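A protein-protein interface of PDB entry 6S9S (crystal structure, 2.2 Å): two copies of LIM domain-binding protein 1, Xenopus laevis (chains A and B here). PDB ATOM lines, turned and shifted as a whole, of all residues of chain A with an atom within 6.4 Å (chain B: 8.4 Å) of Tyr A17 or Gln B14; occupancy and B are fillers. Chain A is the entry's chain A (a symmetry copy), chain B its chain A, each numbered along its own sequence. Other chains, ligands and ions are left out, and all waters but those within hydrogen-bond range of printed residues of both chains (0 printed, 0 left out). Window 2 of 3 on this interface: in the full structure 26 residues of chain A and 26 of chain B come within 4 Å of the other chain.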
ATOM      1  N   GLN A  14     -21.138  23.993  -5.958  1.00  0.00           N
ATOM      2  CA  GLN A  14     -20.535  25.348  -6.114  1.00  0.00           C
ATOM      3  C   GLN A  14     -20.977  25.903  -7.474  1.00  0.00           C
ATOM      4  O   GLN A  14     -20.614  25.300  -8.505  1.00  0.00           O
ATOM      5  CB  GLN A  14     -19.009  25.285  -5.948  1.00  0.00           C
ATOM      6  CG  GLN A  14     -18.359  26.528  -5.334  1.00  0.00           C
ATOM      7  CD  GLN A  14     -19.167  27.269  -4.288  1.00  0.00           C
ATOM      8  OE1 GLN A  14     -20.072  26.701  -3.676  1.00  0.00           O
ATOM      9  NE2 GLN A  14     -18.869  28.545  -4.076  1.00  0.00           N
ATOM     10  N   THR A  15     -21.755  26.989  -7.459  1.00  0.00           N
ATOM     11  CA  THR A  15     -22.356  27.626  -8.656  1.00  0.00           C
ATOM     12  C   THR A  15     -21.271  28.269  -9.517  1.00  0.00           C
ATOM     13  O   THR A  15     -21.373  28.216 -10.757  1.00  0.00           O
ATOM     14  CB  THR A  15     -23.338  28.732  -8.269  1.00  0.00           C
ATOM     15  OG1 THR A  15     -22.583  29.697  -7.535  1.00  0.00           O
ATOM     16  CG2 THR A  15     -24.522  28.218  -7.485  1.00  0.00           C
ATOM     17  N   ASP A  16     -20.308  28.897  -8.852  1.00  0.00           N
ATOM     18  CA  ASP A  16     -19.145  29.600  -9.446  1.00  0.00           C
ATOM     19  C   ASP A  16     -18.377  28.678 -10.395  1.00  0.00           C
ATOM     20  O   ASP A  16     -17.994  29.152 -11.448  1.00  0.00           O
ATOM     21  CB  ASP A  16     -18.219  30.121  -8.339  1.00  0.00           C
ATOM     22  CG  ASP A  16     -18.741  31.370  -7.648  1.00  0.00           C
ATOM     23  OD1 ASP A  16     -19.695  31.259  -6.807  1.00  0.00           O
ATOM     24  OD2 ASP A  16     -18.241  32.449  -8.013  1.00  0.00           O
ATOM     25  N   TYR A  17     -18.132  27.423 -10.036  1.00  0.00           N
ATOM     26  CA  TYR A  17     -17.561  26.427 -10.976  1.00  0.00           C
ATOM     27  C   TYR A  17     -18.414  26.416 -12.271  1.00  0.00           C
ATOM     28  O   TYR A  17     -17.820  26.376 -13.360  1.00  0.00           O
ATOM     29  CB  TYR A  17     -17.454  25.063 -10.292  1.00  0.00           C
ATOM     30  CG  TYR A  17     -16.692  23.990 -11.043  1.00  0.00           C
ATOM     31  CD1 TYR A  17     -15.423  24.211 -11.570  1.00  0.00           C
ATOM     32  CD2 TYR A  17     -17.230  22.714 -11.180  1.00  0.00           C
ATOM     33  CE1 TYR A  17     -14.726  23.200 -12.227  1.00  0.00           C
ATOM     34  CE2 TYR A  17     -16.555  21.699 -11.843  1.00  0.00           C
ATOM     35  CZ  TYR A  17     -15.293  21.936 -12.366  1.00  0.00           C
ATOM     36  OH  TYR A  17     -14.644  20.908 -13.003  1.00  0.00           O
ATOM     37  N   ARG A  18     -19.753  26.488 -12.193  1.00  0.00           N
ATOM     38  CA  ARG A  18     -20.642  26.287 -13.376  1.00  0.00           C
ATOM     39  C   ARG A  18     -20.402  27.402 -14.397  1.00  0.00           C
ATOM     40  O   ARG A  18     -20.403  27.092 -15.594  1.00  0.00           O
ATOM     41  CB  ARG A  18     -22.136  26.204 -13.033  1.00  0.00           C
ATOM     42  CG  ARG A  18     -22.508  25.060 -12.101  1.00  0.00           C
ATOM     43  CD  ARG A  18     -22.284  23.658 -12.641  1.00  0.00           C
ATOM     44  NE  ARG A  18     -23.249  23.308 -13.684  1.00  0.00           N
ATOM     45  CZ  ARG A  18     -22.961  22.988 -14.947  1.00  0.00           C
ATOM     46  NH1 ARG A  18     -21.716  22.928 -15.379  1.00  0.00           N
ATOM     47  NH2 ARG A  18     -23.936  22.703 -15.778  1.00  0.00           N
ATOM     48  N   ILE A  19     -20.181  28.639 -13.952  1.00  0.00           N
ATOM     49  CA  ILE A  19     -19.941  29.795 -14.868  1.00  0.00           C
ATOM     50  C   ILE A  19     -18.496  29.769 -15.361  1.00  0.00           C
ATOM     51  O   ILE A  19     -18.211  30.306 -16.441  1.00  0.00           O
ATOM     52  CB  ILE A  19     -20.286  31.118 -14.189  1.00  0.00           C
ATOM     53  CG1 ILE A  19     -21.738  31.113 -13.702  1.00  0.00           C
ATOM     54  CG2 ILE A  19     -19.993  32.276 -15.140  1.00  0.00           C
ATOM     55  CD1 ILE A  19     -22.741  31.127 -14.824  1.00  0.00           C
ATOM     56  N   PHE A  20     -17.608  29.127 -14.627  1.00  0.00           N
ATOM     57  CA  PHE A  20     -16.249  28.848 -15.139  1.00  0.00           C
ATOM     58  C   PHE A  20     -16.386  27.854 -16.310  1.00  0.00           C
ATOM     59  O   PHE A  20     -15.847  28.138 -17.358  1.00  0.00           O
ATOM     60  CB  PHE A  20     -15.351  28.384 -13.993  1.00  0.00           C
ATOM     61  CG  PHE A  20     -14.210  27.518 -14.416  1.00  0.00           C
ATOM     62  CD1 PHE A  20     -13.016  28.076 -14.842  1.00  0.00           C
ATOM     63  CD2 PHE A  20     -14.345  26.144 -14.400  1.00  0.00           C
ATOM     64  CE1 PHE A  20     -11.973  27.260 -15.274  1.00  0.00           C
ATOM     65  CE2 PHE A  20     -13.311  25.329 -14.842  1.00  0.00           C
ATOM     66  CZ  PHE A  20     -12.123  25.891 -15.269  1.00  0.00           C
ATOM     67  N   GLU A  21     -17.068  26.725 -16.102  1.00  0.00           N
ATOM     68  CA  GLU A  21     -17.314  25.657 -17.104  1.00  0.00           C
ATOM     69  C   GLU A  21     -18.003  26.245 -18.351  1.00  0.00           C
ATOM     70  O   GLU A  21     -17.573  25.902 -19.441  1.00  0.00           O
ATOM     71  CB  GLU A  21     -18.149  24.532 -16.492  1.00  0.00           C
ATOM     72  CG  GLU A  21     -17.342  23.390 -15.930  1.00  0.00           C
ATOM     73  CD  GLU A  21     -18.235  22.340 -15.292  1.00  0.00           C
ATOM     74  OE1 GLU A  21     -18.910  22.694 -14.274  1.00  0.00           O
ATOM     75  OE2 GLU A  21     -18.288  21.165 -15.826  1.00  0.00           O
ATOM     76  N   LEU A  22     -18.996  27.124 -18.164  1.00  0.00           N
ATOM     77  CA  LEU A  22     -19.676  27.890 -19.231  1.00  0.00           C
ATOM     78  C   LEU A  22     -18.665  28.744 -19.992  1.00  0.00           C
ATOM     79  O   LEU A  22     -18.695  28.723 -21.221  1.00  0.00           O
ATOM     80  CB  LEU A  22     -20.783  28.752 -18.623  1.00  0.00           C
ATOM     81  CG  LEU A  22     -21.763  29.358 -19.630  1.00  0.00           C
ATOM     82  CD1 LEU A  22     -23.187  29.200 -19.171  1.00  0.00           C
ATOM     83  CD2 LEU A  22     -21.471  30.823 -19.881  1.00  0.00           C
ATOM     84  N   LYS A  24     -15.554  28.264 -20.196  1.00  0.00           N
ATOM     85  CA  LYS A  24     -14.607  27.286 -20.782  1.00  0.00           C
ATOM     86  C   LYS A  24     -15.196  26.705 -22.094  1.00  0.00           C
ATOM     87  O   LYS A  24     -14.456  26.518 -23.061  1.00  0.00           O
ATOM     88  CB  LYS A  24     -14.319  26.131 -19.826  1.00  0.00           C
ATOM     89  CG  LYS A  24     -12.940  25.568 -20.057  1.00  0.00           C
ATOM     90  CD  LYS A  24     -12.651  24.249 -19.460  1.00  0.00           C
ATOM     91  CE  LYS A  24     -11.246  23.847 -19.857  1.00  0.00           C
ATOM     92  NZ  LYS A  24     -10.728  22.768 -18.992  1.00  0.00           N
ATOM     93  N   GLN B  14      -9.254  18.618 -10.561  1.00  0.00           N
ATOM     94  CA  GLN B  14      -9.358  19.515 -11.748  1.00  0.00           C
ATOM     95  C   GLN B  14      -8.516  20.765 -11.464  1.00  0.00           C
ATOM     96  O   GLN B  14      -8.850  21.500 -10.511  1.00  0.00           O
ATOM     97  CB  GLN B  14     -10.828  19.829 -12.063  1.00  0.00           C
ATOM     98  CG  GLN B  14     -11.157  20.039 -13.544  1.00  0.00           C
ATOM     99  CD  GLN B  14     -10.368  19.211 -14.537  1.00  0.00           C
ATOM    100  OE1 GLN B  14      -9.820  18.165 -14.187  1.00  0.00           O
ATOM    101  NE2 GLN B  14     -10.283  19.667 -15.781  1.00  0.00           N
ATOM    102  N   THR B  15      -7.453  20.968 -12.247  1.00  0.00           N
ATOM    103  CA  THR B  15      -6.468  22.065 -12.084  1.00  0.00           C
ATOM    104  C   THR B  15      -7.112  23.411 -12.408  1.00  0.00           C
ATOM    105  O   THR B  15      -6.801  24.409 -11.731  1.00  0.00           O
ATOM    106  CB  THR B  15      -5.278  21.896 -13.029  1.00  0.00           C
ATOM    107  OG1 THR B  15      -5.814  21.920 -14.352  1.00  0.00           O
ATOM    108  CG2 THR B  15      -4.486  20.639 -12.758  1.00  0.00           C
ATOM    109  N   ASP B  16      -7.935  23.417 -13.451  1.00  0.00           N
ATOM    110  CA  ASP B  16      -8.684  24.585 -13.973  1.00  0.00           C
ATOM    111  C   ASP B  16      -9.510  25.242 -12.866  1.00  0.00           C
ATOM    112  O   ASP B  16      -9.519  26.458 -12.820  1.00  0.00           O
ATOM    113  CB  ASP B  16      -9.588  24.159 -15.136  1.00  0.00           C
ATOM    114  CG  ASP B  16      -8.839  23.938 -16.440  1.00  0.00           C
ATOM    115  OD1 ASP B  16      -8.145  22.876 -16.581  1.00  0.00           O
ATOM    116  OD2 ASP B  16      -8.895  24.863 -17.269  1.00  0.00           O
ATOM    117  N   TYR B  17     -10.202  24.483 -12.023  1.00  0.00           N
ATOM    118  CA  TYR B  17     -10.870  25.038 -10.820  1.00  0.00           C
ATOM    119  C   TYR B  17      -9.836  25.864 -10.011  1.00  0.00           C
ATOM    120  O   TYR B  17     -10.197  26.959  -9.551  1.00  0.00           O
ATOM    121  CB  TYR B  17     -11.528  23.913 -10.021  1.00  0.00           C
ATOM    122  CG  TYR B  17     -12.434  24.334  -8.882  1.00  0.00           C
ATOM    123  CD1 TYR B  17     -13.446  25.276  -9.048  1.00  0.00           C
ATOM    124  CD2 TYR B  17     -12.310  23.741  -7.630  1.00  0.00           C
ATOM    125  CE1 TYR B  17     -14.290  25.625  -7.997  1.00  0.00           C
ATOM    126  CE2 TYR B  17     -13.134  24.086  -6.568  1.00  0.00           C
ATOM    127  CZ  TYR B  17     -14.134  25.028  -6.748  1.00  0.00           C
ATOM    128  OH  TYR B  17     -14.943  25.337  -5.682  1.00  0.00           O
ATOM    129  N   ARG B  18      -8.583  25.406  -9.860  1.00  0.00           N
ATOM    130  CA  ARG B  18      -7.597  26.044  -8.937  1.00  0.00           C
ATOM    131  C   ARG B  18      -7.277  27.459  -9.424  1.00  0.00           C
ATOM    132  O   ARG B  18      -7.148  28.344  -8.570  1.00  0.00           O
ATOM    133  CB  ARG B  18      -6.298  25.247  -8.756  1.00  0.00           C
ATOM    134  CG  ARG B  18      -6.488  23.853  -8.175  1.00  0.00           C
ATOM    135  CD  ARG B  18      -7.037  23.787  -6.760  1.00  0.00           C
ATOM    136  NE  ARG B  18      -6.054  24.220  -5.766  1.00  0.00           N
ATOM    137  CZ  ARG B  18      -6.186  25.247  -4.925  1.00  0.00           C
ATOM    138  NH1 ARG B  18      -7.280  25.982  -4.895  1.00  0.00           N
ATOM    139  NH2 ARG B  18      -5.212  25.525  -4.089  1.00  0.00           N
ATOM    140  N   ILE B  19      -7.176  27.677 -10.736  1.00  0.00           N
ATOM    141  CA  ILE B  19      -6.863  29.020 -11.310  1.00  0.00           C
ATOM    142  C   ILE B  19      -8.122  29.883 -11.316  1.00  0.00           C
ATOM    143  O   ILE B  19      -8.015  31.118 -11.292  1.00  0.00           O
ATOM    144  CB  ILE B  19      -6.252  28.895 -12.704  1.00  0.00           C
ATOM    145  CG1 ILE B  19      -4.994  28.023 -12.667  1.00  0.00           C
ATOM    146  CG2 ILE B  19      -5.980  30.287 -13.272  1.00  0.00           C
ATOM    147  CD1 ILE B  19      -3.846  28.665 -11.936  1.00  0.00           C
ATOM    148  N   PHE B  20      -9.289  29.268 -11.300  1.00  0.00           N
ATOM    149  CA  PHE B  20     -10.544  30.012 -11.066  1.00  0.00           C
ATOM    150  C   PHE B  20     -10.510  30.542  -9.618  1.00  0.00           C
ATOM    151  O   PHE B  20     -10.725  31.722  -9.443  1.00  0.00           O
ATOM    152  CB  PHE B  20     -11.741  29.126 -11.408  1.00  0.00           C
ATOM    153  CG  PHE B  20     -12.996  29.478 -10.678  1.00  0.00           C
ATOM    154  CD1 PHE B  20     -13.851  30.453 -11.165  1.00  0.00           C
ATOM    155  CD2 PHE B  20     -13.307  28.838  -9.494  1.00  0.00           C
ATOM    156  CE1 PHE B  20     -14.997  30.802 -10.455  1.00  0.00           C
ATOM    157  CE2 PHE B  20     -14.443  29.194  -8.778  1.00  0.00           C
ATOM    158  CZ  PHE B  20     -15.290  30.170  -9.267  1.00  0.00           C
ATOM    159  N   GLU B  21     -10.272  29.671  -8.635  1.00  0.00           N
ATOM    160  CA  GLU B  21     -10.191  29.992  -7.186  1.00  0.00           C
ATOM    161  C   GLU B  21      -9.130  31.082  -6.940  1.00  0.00           C
ATOM    162  O   GLU B  21      -9.433  31.997  -6.191  1.00  0.00           O
ATOM    163  CB  GLU B  21      -9.884  28.731  -6.377  1.00  0.00           C
ATOM    164  CG  GLU B  21     -11.101  28.025  -5.836  1.00  0.00           C
ATOM    165  CD  GLU B  21     -10.721  26.756  -5.092  1.00  0.00           C
ATOM    166  OE1 GLU B  21     -10.173  25.829  -5.769  1.00  0.00           O
ATOM    167  OE2 GLU B  21     -10.941  26.694  -3.822  1.00  0.00           O
ATOM    168  N   LYS B  24     -10.424  34.277  -8.203  1.00  0.00           N
ATOM    169  CA  LYS B  24     -11.504  34.658  -7.261  1.00  0.00           C
ATOM    170  C   LYS B  24     -10.892  35.340  -6.009  1.00  0.00           C
ATOM    171  O   LYS B  24     -11.458  36.314  -5.511  1.00  0.00           O
ATOM    172  CB  LYS B  24     -12.315  33.447  -6.807  1.00  0.00           C
ATOM    173  CG  LYS B  24     -13.732  33.839  -6.474  1.00  0.00           C
ATOM    174  CD  LYS B  24     -14.529  32.865  -5.704  1.00  0.00           C
ATOM    175  CE  LYS B  24     -15.888  33.474  -5.430  1.00  0.00           C
ATOM    176  NZ  LYS B  24     -16.873  32.445  -5.039  1.00  0.00           N
ATOM    177  N   PRO B  94      -6.089  24.912 -22.038  1.00  0.00           N
ATOM    178  CA  PRO B  94      -4.990  24.264 -21.321  1.00  0.00           C
ATOM    179  C   PRO B  94      -5.009  22.722 -21.380  1.00  0.00           C
ATOM    180  O   PRO B  94      -6.090  22.160 -21.214  1.00  0.00           O
ATOM    181  CB  PRO B  94      -5.194  24.707 -19.852  1.00  0.00           C
ATOM    182  CG  PRO B  94      -6.660  25.090 -19.735  1.00  0.00           C
ATOM    183  CD  PRO B  94      -7.016  25.604 -21.120  1.00  0.00           C
ATOM    184  N   LYS B  95      -3.806  22.120 -21.511  1.00  0.00           N
ATOM    185  CA  LYS B  95      -3.498  20.657 -21.455  1.00  0.00           C
ATOM    186  C   LYS B  95      -3.186  20.194 -20.013  1.00  0.00           C
ATOM    187  O   LYS B  95      -2.045  20.409 -19.520  1.00  0.00           O
ATOM    188  CB  LYS B  95      -2.254  20.290 -22.284  1.00  0.00           C
ATOM    189  CG  LYS B  95      -2.050  20.974 -23.641  1.00  0.00           C
ATOM    190  CD  LYS B  95      -0.549  21.043 -24.071  1.00  0.00           C
ATOM    191  CE  LYS B  95      -0.222  22.086 -25.129  1.00  0.00           C
ATOM    192  NZ  LYS B  95      -0.579  21.604 -26.487  1.00  0.00           N
ATOM    193  N   GLU B  96      -4.123  19.485 -19.381  1.00  0.00           N
ATOM    194  CA  GLU B  96      -3.885  18.760 -18.103  1.00  0.00           C
ATOM    195  C   GLU B  96      -3.153  17.445 -18.446  1.00  0.00           C
ATOM    196  O   GLU B  96      -3.653  16.756 -19.293  1.00  0.00           O
ATOM    197  CB  GLU B  96      -5.252  18.604 -17.421  1.00  0.00           C
ATOM    198  CG  GLU B  96      -5.199  18.348 -15.922  1.00  0.00           C
ATOM    199  CD  GLU B  96      -6.554  18.407 -15.232  1.00  0.00           C
ATOM    200  OE1 GLU B  96      -6.872  19.466 -14.672  1.00  0.00           O
ATOM    201  OE2 GLU B  96      -7.309  17.398 -15.264  1.00  0.00           O
ATOM    202  N   PHE B  98      -1.105  13.993 -16.226  1.00  0.00           N
ATOM    203  CA  PHE B  98      -0.850  13.356 -14.905  1.00  0.00           C
ATOM    204  C   PHE B  98       0.498  12.625 -14.936  1.00  0.00           C
ATOM    205  O   PHE B  98       0.893  12.145 -16.004  1.00  0.00           O
ATOM    206  CB  PHE B  98      -2.017  12.447 -14.505  1.00  0.00           C
ATOM    207  CG  PHE B  98      -3.285  13.191 -14.161  1.00  0.00           C
ATOM    208  CD1 PHE B  98      -4.162  13.605 -15.155  1.00  0.00           C
ATOM    209  CD2 PHE B  98      -3.589  13.525 -12.845  1.00  0.00           C
ATOM    210  CE1 PHE B  98      -5.315  14.321 -14.842  1.00  0.00           C
ATOM    211  CE2 PHE B  98      -4.743  14.237 -12.535  1.00  0.00           C
ATOM    212  CZ  PHE B  98      -5.607  14.635 -13.529  1.00  0.00           C
ATOM    213  N   VAL B 103       0.577  16.889 -11.240  1.00  0.00           N
ATOM    214  CA  VAL B 103      -0.220  17.199 -12.473  1.00  0.00           C
ATOM    215  C   VAL B 103       0.424  18.403 -13.159  1.00  0.00           C
ATOM    216  O   VAL B 103       0.648  19.397 -12.455  1.00  0.00           O
ATOM    217  CB  VAL B 103      -1.676  17.576 -12.139  1.00  0.00           C
ATOM    218  CG1 VAL B 103      -2.504  17.758 -13.397  1.00  0.00           C
ATOM    219  CG2 VAL B 103      -2.331  16.593 -11.186  1.00  0.00           C
ATOM    220  N   LEU B 105      -0.097  21.445 -16.216  1.00  0.00           N
ATOM    221  CA  LEU B 105      -1.108  22.271 -16.908  1.00  0.00           C
ATOM    222  C   LEU B 105      -0.278  23.182 -17.803  1.00  0.00           C
ATOM    223  O   LEU B 105       0.440  24.015 -17.253  1.00  0.00           O
ATOM    224  CB  LEU B 105      -1.950  23.030 -15.871  1.00  0.00           C
ATOM    225  CG  LEU B 105      -3.011  24.004 -16.389  1.00  0.00           C
ATOM    226  CD1 LEU B 105      -4.066  24.281 -15.341  1.00  0.00           C
ATOM    227  CD2 LEU B 105      -2.402  25.319 -16.826  1.00  0.00           C
ATOM    228  N   PHE B 134       1.323  21.041 -10.228  1.00  0.00           N
ATOM    229  CA  PHE B 134       0.562  21.067  -8.960  1.00  0.00           C
ATOM    230  C   PHE B 134       0.838  19.780  -8.197  1.00  0.00           C
ATOM    231  O   PHE B 134       0.909  18.732  -8.804  1.00  0.00           O
ATOM    232  CB  PHE B 134      -0.947  21.111  -9.168  1.00  0.00           C
ATOM    233  CG  PHE B 134      -1.484  22.326  -9.869  1.00  0.00           C
ATOM    234  CD1 PHE B 134      -1.237  22.530 -11.216  1.00  0.00           C
ATOM    235  CD2 PHE B 134      -2.307  23.222  -9.196  1.00  0.00           C
ATOM    236  CE1 PHE B 134      -1.758  23.637 -11.867  1.00  0.00           C
ATOM    237  CE2 PHE B 134      -2.846  24.318  -9.849  1.00  0.00           C
ATOM    238  CZ  PHE B 134      -2.572  24.518 -11.187  1.00  0.00           C
ATOM    239  N   PHE B 136      -0.350  16.714  -6.401  1.00  0.00           N
ATOM    240  CA  PHE B 136      -1.590  15.897  -6.471  1.00  0.00           C
ATOM    241  C   PHE B 136      -1.872  15.384  -5.060  1.00  0.00           C
ATOM    242  O   PHE B 136      -1.550  14.228  -4.790  1.00  0.00           O
ATOM    243  CB  PHE B 136      -1.519  14.779  -7.523  1.00  0.00           C
ATOM    244  CG  PHE B 136      -2.818  14.014  -7.682  1.00  0.00           C
ATOM    245  CD1 PHE B 136      -3.946  14.625  -8.223  1.00  0.00           C
ATOM    246  CD2 PHE B 136      -2.938  12.697  -7.247  1.00  0.00           C
ATOM    247  CE1 PHE B 136      -5.147  13.936  -8.346  1.00  0.00           C
ATOM    248  CE2 PHE B 136      -4.141  12.010  -7.365  1.00  0.00           C
ATOM    249  CZ  PHE B 136      -5.242  12.632  -7.913  1.00  0.00           C
ATOM    250  N   MET B 140      -3.817  20.612  -3.513  1.00  0.00           N
ATOM    251  CA  MET B 140      -3.614  20.900  -4.963  1.00  0.00           C
ATOM    252  C   MET B 140      -2.924  22.258  -5.129  1.00  0.00           C
ATOM    253  O   MET B 140      -3.475  23.127  -5.825  1.00  0.00           O
ATOM    254  CB  MET B 140      -4.948  20.947  -5.712  1.00  0.00           C
ATOM    255  CG  MET B 140      -5.594  19.582  -5.939  1.00  0.00           C
ATOM    256  SD  MET B 140      -4.924  18.674  -7.364  1.00  0.00           S
ATOM    257  CE  MET B 140      -5.431  19.733  -8.719  1.00  0.00           C
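Of chain B, only Gln B14 (3.6 Å) and Tyr B17 (3.4 Å) come within 4 Å of Tyr A17.
Of chain A, only Tyr A17 comes within 4 Å of Gln B14.
Of the printed residues of chain A, Asp B16 touches Phe A20 (3.1 Å) and Lys A24 (3.3 Å).
Of the printed residues of chain B, Gln A14 touches Tyr B17 (3.6 Å).
Val B103 touches none of the printed residues of chain A.
Glu B21 touches none of the printed residues of chain A.
The nearest residue of chain A that does not touch Gln B14 is Lys A24 (4.5 Å).
The nearest printed residue of chain A that does not touch Phe B20 is Tyr A17 (4.03 Å).
Of the 18 printed residues of chain B, 5 touch a printed residue of chain A.
Hydrophobic or aromatic side chains of chain B that line the printed part of chain A: Tyr B17 and Phe B20.
Along chain B the printed residues that touch a printed residue of chain A span positions 14 to 24.
Among the printed residues, Asp or Glu carboxylates within 4 Å of a Lys or Arg side-chain nitrogen of the other chain: Asp A16 with Lys B24 (3.3 Å) and Lys A24 with Asp B16 (3.3 Å).
The side-chain carboxylate of Asp B16 lies within salt-bridge range of the side-chain amino group of Lys A24 (3.3 Å).
The side-chain amino group of Lys B24 is in salt-bridge range of the side-chain carboxylate of Asp A16, 3.3 Å away.
CG of Gln A14 touches OH of Tyr B17, 3.6 Å away.
Asp A16 touches Phe B20.
CG of Gln B14 touches OH of Tyr A17, at 3.6 Å.
CD1 of Tyr B17 touches CD1 of Tyr A17 (3.4 Å).
Phe A20 touches Asp B16 (CZ to CB, 3.1 Å).
Phe A20 touches Phe B20.
Gln A14 touches Tyr B17, and with the chains exchanged Tyr A17 touches Gln B14.
Asp A16 touches Lys B24, and with the chains exchanged Lys A24 touches Asp B16.
Tyr A17 touches its own counterpart, Tyr B17.
Phe B20 touches its own counterpart, Phe A20.
9 positions are printed for both chains.
OE2 of Glu B96 sits close to OE1 of Gln B14 (2.8 Å).
OG1 of Thr A15 sits at hydrogen-bond distance from OD1 of Asp A16, at 3.4 Å.
The side-chain hydroxyl (OG1) of Thr B15 lies within hydrogen-bond range of the side-chain carboxylate (OD1) of Asp B16 (3.4 Å).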
